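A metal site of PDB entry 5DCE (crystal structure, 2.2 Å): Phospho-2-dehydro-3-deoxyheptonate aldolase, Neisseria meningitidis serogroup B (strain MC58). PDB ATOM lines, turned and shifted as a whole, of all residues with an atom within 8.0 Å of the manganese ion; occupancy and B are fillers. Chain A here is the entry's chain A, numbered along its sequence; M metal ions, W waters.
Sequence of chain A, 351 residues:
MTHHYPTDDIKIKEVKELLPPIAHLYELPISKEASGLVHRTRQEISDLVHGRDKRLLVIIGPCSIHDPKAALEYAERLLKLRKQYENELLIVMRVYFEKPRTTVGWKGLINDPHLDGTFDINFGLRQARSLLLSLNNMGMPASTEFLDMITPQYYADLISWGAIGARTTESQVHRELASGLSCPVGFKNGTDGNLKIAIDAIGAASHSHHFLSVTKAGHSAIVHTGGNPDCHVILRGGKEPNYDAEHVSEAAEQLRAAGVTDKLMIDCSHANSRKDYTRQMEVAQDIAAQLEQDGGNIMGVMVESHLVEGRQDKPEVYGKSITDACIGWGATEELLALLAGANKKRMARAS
Of the 21 residues printed, 4 come within 4 Å of the manganese ion. The nearest printed residue that does not touch the manganese ion is Arg 94 (4.3 Å).
SG of Cys 326 is in hydrogen-bond range of O of Asp 324 (3.6 Å). The side-chain hydroxyl of Ser 321 lies within hydrogen-bond range of the backbone carbonyl oxygen of Asp 324 (2.6 Å). OE2 of Glu 304 lies close to NH2 of Arg 94 (3.5 Å). OG of Ser 269 lies within hydrogen-bond range of OE1 of Glu 304, at 2.7 Å. A ring nitrogen (ND1) of His 270 lies within hydrogen-bond range of the side-chain carboxylate of Asp 267 (2.7 Å). The backbone carbonyl oxygen of Cys 63 sits at hydrogen-bond distance from the guanidinium group of Arg 94 (2.8 Å). The side-chain sulfur (SG) of Cys 63 sits close to the side-chain hydroxyl (OG1) of Thr 323. N of Cys 63 is in hydrogen-bond range of SG of Cys 326, at 3.6 Å.
The manganese ion is bound by OD2 of Asp 324 (1.8 Å), water W1 (2.0 Å), OE2 of Glu 304 (2.0 Å), NE2 of His 270 (2.4 Å) and SG of Cys 63 (2.6 Å).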
ATOM      1  N   GLY A  61      -2.794  24.884  16.629  1.00  0.00           N
ATOM      2  CA  GLY A  61      -3.674  23.737  16.585  1.00  0.00           C
ATOM      3  C   GLY A  61      -4.278  23.358  17.934  1.00  0.00           C
ATOM      4  O   GLY A  61      -4.183  24.100  18.904  1.00  0.00           O
ATOM      5  N   PRO A  62      -4.899  22.195  18.019  1.00  0.00           N
ATOM      6  CA  PRO A  62      -5.567  21.857  19.252  1.00  0.00           C
ATOM      7  C   PRO A  62      -4.645  21.809  20.469  1.00  0.00           C
ATOM      8  O   PRO A  62      -3.455  21.580  20.338  1.00  0.00           O
ATOM      9  CB  PRO A  62      -6.158  20.497  18.967  1.00  0.00           C
ATOM     10  CG  PRO A  62      -6.456  20.536  17.490  1.00  0.00           C
ATOM     11  CD  PRO A  62      -5.350  21.364  16.891  1.00  0.00           C
ATOM     12  N   CYS A  63      -5.224  22.053  21.631  1.00  0.00           N
ATOM     13  CA  CYS A  63      -4.525  21.816  22.873  1.00  0.00           C
ATOM     14  C   CYS A  63      -4.077  20.357  22.877  1.00  0.00           C
ATOM     15  O   CYS A  63      -2.900  20.080  23.039  1.00  0.00           O
ATOM     16  CB  CYS A  63      -5.420  22.083  24.069  1.00  0.00           C
ATOM     17  SG  CYS A  63      -4.669  21.632  25.651  1.00  0.00           S
ATOM     18  N   SER A  64      -5.019  19.450  22.654  1.00  0.00           N
ATOM     19  CA  SER A  64      -4.721  18.024  22.473  1.00  0.00           C
ATOM     20  C   SER A  64      -5.553  17.507  21.328  1.00  0.00           C
ATOM     21  O   SER A  64      -6.628  18.051  21.028  1.00  0.00           O
ATOM     22  CB  SER A  64      -5.088  17.223  23.702  1.00  0.00           C
ATOM     23  OG  SER A  64      -6.450  17.425  24.057  1.00  0.00           O
ATOM     24  N   ARG A  94       0.025  21.955  15.706  1.00  0.00           N
ATOM     25  CA  ARG A  94       0.093  21.334  17.001  1.00  0.00           C
ATOM     26  C   ARG A  94      -0.578  19.996  16.940  1.00  0.00           C
ATOM     27  O   ARG A  94      -1.779  19.922  16.688  1.00  0.00           O
ATOM     28  CB  ARG A  94      -0.702  22.142  18.004  1.00  0.00           C
ATOM     29  CG  ARG A  94       0.031  23.226  18.719  1.00  0.00           C
ATOM     30  CD  ARG A  94      -0.908  23.816  19.766  1.00  0.00           C
ATOM     31  NE  ARG A  94      -1.170  22.909  20.878  1.00  0.00           N
ATOM     32  CZ  ARG A  94      -0.559  22.956  22.061  1.00  0.00           C
ATOM     33  NH1 ARG A  94       0.406  23.839  22.302  1.00  0.00           N
ATOM     34  NH2 ARG A  94      -0.889  22.092  22.993  1.00  0.00           N
ATOM     35  N   TYR A  96      -0.502  17.495  19.733  1.00  0.00           N
ATOM     36  CA  TYR A  96      -0.138  17.076  21.075  1.00  0.00           C
ATOM     37  C   TYR A  96      -1.107  16.001  21.513  1.00  0.00           C
ATOM     38  O   TYR A  96      -2.309  16.189  21.408  1.00  0.00           O
ATOM     39  CB  TYR A  96      -0.295  18.218  22.053  1.00  0.00           C
ATOM     40  CG  TYR A  96       0.782  19.231  22.026  1.00  0.00           C
ATOM     41  CD1 TYR A  96       1.338  19.656  20.835  1.00  0.00           C
ATOM     42  CD2 TYR A  96       1.235  19.821  23.226  1.00  0.00           C
ATOM     43  CE1 TYR A  96       2.338  20.628  20.821  1.00  0.00           C
ATOM     44  CE2 TYR A  96       2.215  20.800  23.217  1.00  0.00           C
ATOM     45  CZ  TYR A  96       2.764  21.193  22.016  1.00  0.00           C
ATOM     46  OH  TYR A  96       3.756  22.153  21.967  1.00  0.00           O
ATOM     47  N   GLU A  98      -1.336  14.466  24.671  1.00  0.00           N
ATOM     48  CA  GLU A  98      -1.734  14.524  26.086  1.00  0.00           C
ATOM     49  C   GLU A  98      -1.388  15.855  26.744  1.00  0.00           C
ATOM     50  O   GLU A  98      -0.223  16.279  26.692  1.00  0.00           O
ATOM     51  CB  GLU A  98      -1.018  13.433  26.870  1.00  0.00           C
ATOM     52  CG  GLU A  98      -1.437  13.326  28.330  1.00  0.00           C
ATOM     53  CD  GLU A  98      -0.621  12.280  29.094  1.00  0.00           C
ATOM     54  OE1 GLU A  98      -0.966  11.965  30.265  1.00  0.00           O
ATOM     55  OE2 GLU A  98       0.347  11.761  28.516  1.00  0.00           O
ATOM     56  N   LYS A  99      -2.390  16.482  27.362  1.00  0.00           N
ATOM     57  CA  LYS A  99      -2.192  17.526  28.360  1.00  0.00           C
ATOM     58  C   LYS A  99      -1.809  16.896  29.720  1.00  0.00           C
ATOM     59  O   LYS A  99      -2.644  16.220  30.343  1.00  0.00           O
ATOM     60  CB  LYS A  99      -3.469  18.356  28.529  1.00  0.00           C
ATOM     61  N   PRO A 100      -0.557  17.102  30.182  1.00  0.00           N
ATOM     62  CA  PRO A 100      -0.222  16.663  31.548  1.00  0.00           C
ATOM     63  C   PRO A 100      -1.169  17.276  32.591  1.00  0.00           C
ATOM     64  O   PRO A 100      -1.464  18.455  32.517  1.00  0.00           O
ATOM     65  CB  PRO A 100       1.227  17.134  31.744  1.00  0.00           C
ATOM     66  CG  PRO A 100       1.472  18.158  30.687  1.00  0.00           C
ATOM     67  CD  PRO A 100       0.588  17.757  29.531  1.00  0.00           C
ATOM     68  N   GLU A 145       4.566  17.682  22.107  1.00  0.00           N
ATOM     69  CA  GLU A 145       5.330  17.707  23.339  1.00  0.00           C
ATOM     70  C   GLU A 145       5.677  16.291  23.672  1.00  0.00           C
ATOM     71  O   GLU A 145       4.807  15.422  23.766  1.00  0.00           O
ATOM     72  CB  GLU A 145       4.564  18.314  24.515  1.00  0.00           C
ATOM     73  CG  GLU A 145       5.314  18.127  25.836  1.00  0.00           C
ATOM     74  CD  GLU A 145       4.639  18.729  27.065  1.00  0.00           C
ATOM     75  OE1 GLU A 145       3.610  19.383  26.964  1.00  0.00           O
ATOM     76  OE2 GLU A 145       5.208  18.584  28.147  1.00  0.00           O
ATOM     77  N   LYS A 188       9.698  25.632  27.731  1.00  0.00           N
ATOM     78  CA  LYS A 188       8.864  26.617  28.378  1.00  0.00           C
ATOM     79  C   LYS A 188       9.431  27.103  29.709  1.00  0.00           C
ATOM     80  O   LYS A 188      10.035  26.316  30.445  1.00  0.00           O
ATOM     81  CB  LYS A 188       7.486  26.020  28.594  1.00  0.00           C
ATOM     82  CG  LYS A 188       6.734  25.940  27.292  1.00  0.00           C
ATOM     83  CD  LYS A 188       5.284  25.540  27.442  1.00  0.00           C
ATOM     84  CE  LYS A 188       4.488  26.139  26.295  1.00  0.00           C
ATOM     85  NZ  LYS A 188       3.026  25.950  26.435  1.00  0.00           N
ATOM     86  N   ASP A 267       3.979  32.176  23.694  1.00  0.00           N
ATOM     87  CA  ASP A 267       2.782  31.376  23.687  1.00  0.00           C
ATOM     88  C   ASP A 267       1.635  32.320  24.005  1.00  0.00           C
ATOM     89  O   ASP A 267       1.582  32.927  25.072  1.00  0.00           O
ATOM     90  CB  ASP A 267       2.938  30.259  24.736  1.00  0.00           C
ATOM     91  CG  ASP A 267       1.744  29.347  24.824  1.00  0.00           C
ATOM     92  OD1 ASP A 267       0.756  29.587  24.092  1.00  0.00           O
ATOM     93  OD2 ASP A 267       1.779  28.409  25.673  1.00  0.00           O
ATOM     94  N   SER A 269      -1.295  31.443  24.652  1.00  0.00           N
ATOM     95  CA  SER A 269      -2.274  30.729  25.472  1.00  0.00           C
ATOM     96  C   SER A 269      -1.779  30.510  26.915  1.00  0.00           C
ATOM     97  O   SER A 269      -0.947  31.267  27.416  1.00  0.00           O
ATOM     98  CB  SER A 269      -2.663  29.399  24.814  1.00  0.00           C
ATOM     99  OG  SER A 269      -3.978  28.949  25.217  1.00  0.00           O
ATOM    100  N   HIS A 270      -2.342  29.499  27.572  1.00  0.00           N
ATOM    101  CA  HIS A 270      -2.017  29.136  28.941  1.00  0.00           C
ATOM    102  C   HIS A 270      -1.952  30.340  29.884  1.00  0.00           C
ATOM    103  O   HIS A 270      -2.955  31.036  30.035  1.00  0.00           O
ATOM    104  CB  HIS A 270      -0.781  28.236  28.939  1.00  0.00           C
ATOM    105  CG  HIS A 270      -0.945  27.079  28.008  1.00  0.00           C
ATOM    106  ND1 HIS A 270      -0.303  27.019  26.791  1.00  0.00           N
ATOM    107  CD2 HIS A 270      -1.755  26.002  28.070  1.00  0.00           C
ATOM    108  CE1 HIS A 270      -0.698  25.932  26.146  1.00  0.00           C
ATOM    109  NE2 HIS A 270      -1.593  25.311  26.896  1.00  0.00           N
ATOM    110  N   MET A 302       2.797  30.618  19.653  1.00  0.00           N
ATOM    111  CA  MET A 302       2.047  29.398  19.837  1.00  0.00           C
ATOM    112  C   MET A 302       0.614  29.822  20.086  1.00  0.00           C
ATOM    113  O   MET A 302       0.357  30.790  20.773  1.00  0.00           O
ATOM    114  CB  MET A 302       2.616  28.622  21.015  1.00  0.00           C
ATOM    115  CG  MET A 302       2.058  27.242  21.226  1.00  0.00           C
ATOM    116  SD  MET A 302       2.906  26.337  22.585  1.00  0.00           S
ATOM    117  CE  MET A 302       4.591  26.798  22.265  1.00  0.00           C
ATOM    118  N   GLU A 304      -3.454  28.126  20.630  1.00  0.00           N
ATOM    119  CA  GLU A 304      -4.321  26.952  20.777  1.00  0.00           C
ATOM    120  C   GLU A 304      -5.605  27.234  20.034  1.00  0.00           C
ATOM    121  O   GLU A 304      -6.375  28.122  20.410  1.00  0.00           O
ATOM    122  CB  GLU A 304      -4.553  26.629  22.237  1.00  0.00           C
ATOM    123  CG  GLU A 304      -3.269  26.159  22.908  1.00  0.00           C
ATOM    124  CD  GLU A 304      -3.522  25.576  24.257  1.00  0.00           C
ATOM    125  OE1 GLU A 304      -4.175  26.269  25.079  1.00  0.00           O
ATOM    126  OE2 GLU A 304      -3.074  24.435  24.507  1.00  0.00           O
ATOM    127  N   SER A 321     -12.212  21.178  21.538  1.00  0.00           N
ATOM    128  CA  SER A 321     -11.265  20.688  22.557  1.00  0.00           C
ATOM    129  C   SER A 321     -11.907  20.110  23.827  1.00  0.00           C
ATOM    130  O   SER A 321     -12.887  20.622  24.335  1.00  0.00           O
ATOM    131  CB  SER A 321     -10.307  21.816  22.962  1.00  0.00           C
ATOM    132  OG  SER A 321      -9.473  21.382  24.021  1.00  0.00           O
ATOM    133  N   THR A 323      -9.533  19.426  26.308  1.00  0.00           N
ATOM    134  CA  THR A 323      -8.576  19.937  27.270  1.00  0.00           C
ATOM    135  C   THR A 323      -8.715  21.454  27.355  1.00  0.00           C
ATOM    136  O   THR A 323      -9.800  21.911  27.654  1.00  0.00           O
ATOM    137  CB  THR A 323      -7.148  19.395  26.989  1.00  0.00           C
ATOM    138  OG1 THR A 323      -6.804  19.545  25.614  1.00  0.00           O
ATOM    139  CG2 THR A 323      -7.106  17.903  27.335  1.00  0.00           C
ATOM    140  N   ASP A 324      -7.663  22.236  27.127  1.00  0.00           N
ATOM    141  CA  ASP A 324      -7.766  23.722  27.203  1.00  0.00           C
ATOM    142  C   ASP A 324      -8.662  24.248  26.086  1.00  0.00           C
ATOM    143  O   ASP A 324      -8.735  23.660  25.000  1.00  0.00           O
ATOM    144  CB  ASP A 324      -6.400  24.405  27.059  1.00  0.00           C
ATOM    145  CG  ASP A 324      -5.382  23.946  28.124  1.00  0.00           C
ATOM    146  OD1 ASP A 324      -5.811  23.669  29.267  1.00  0.00           O
ATOM    147  OD2 ASP A 324      -4.165  23.836  27.789  1.00  0.00           O
ATOM    148  N   ALA A 325      -9.304  25.370  26.365  1.00  0.00           N
ATOM    149  CA  ALA A 325     -10.226  25.982  25.443  1.00  0.00           C
ATOM    150  C   ALA A 325      -9.462  26.612  24.310  1.00  0.00           C
ATOM    151  O   ALA A 325      -8.479  27.300  24.531  1.00  0.00           O
ATOM    152  CB  ALA A 325     -11.065  27.019  26.153  1.00  0.00           C
ATOM    153  N   CYS A 326      -9.905  26.381  23.093  1.00  0.00           N
ATOM    154  CA  CYS A 326      -9.202  26.911  21.952  1.00  0.00           C
ATOM    155  C   CYS A 326     -10.052  27.961  21.302  1.00  0.00           C
ATOM    156  O   CYS A 326     -11.258  28.000  21.526  1.00  0.00           O
ATOM    157  CB  CYS A 326      -8.923  25.788  20.960  1.00  0.00           C
ATOM    158  SG  CYS A 326      -7.857  24.501  21.650  1.00  0.00           S
HETATM  159 MN    MN M   1      -3.114  23.588  26.357  1.00  0.00          MN
HETATM  160  O   HOH W   1      -1.912  22.107  27.028  1.00  0.00           O
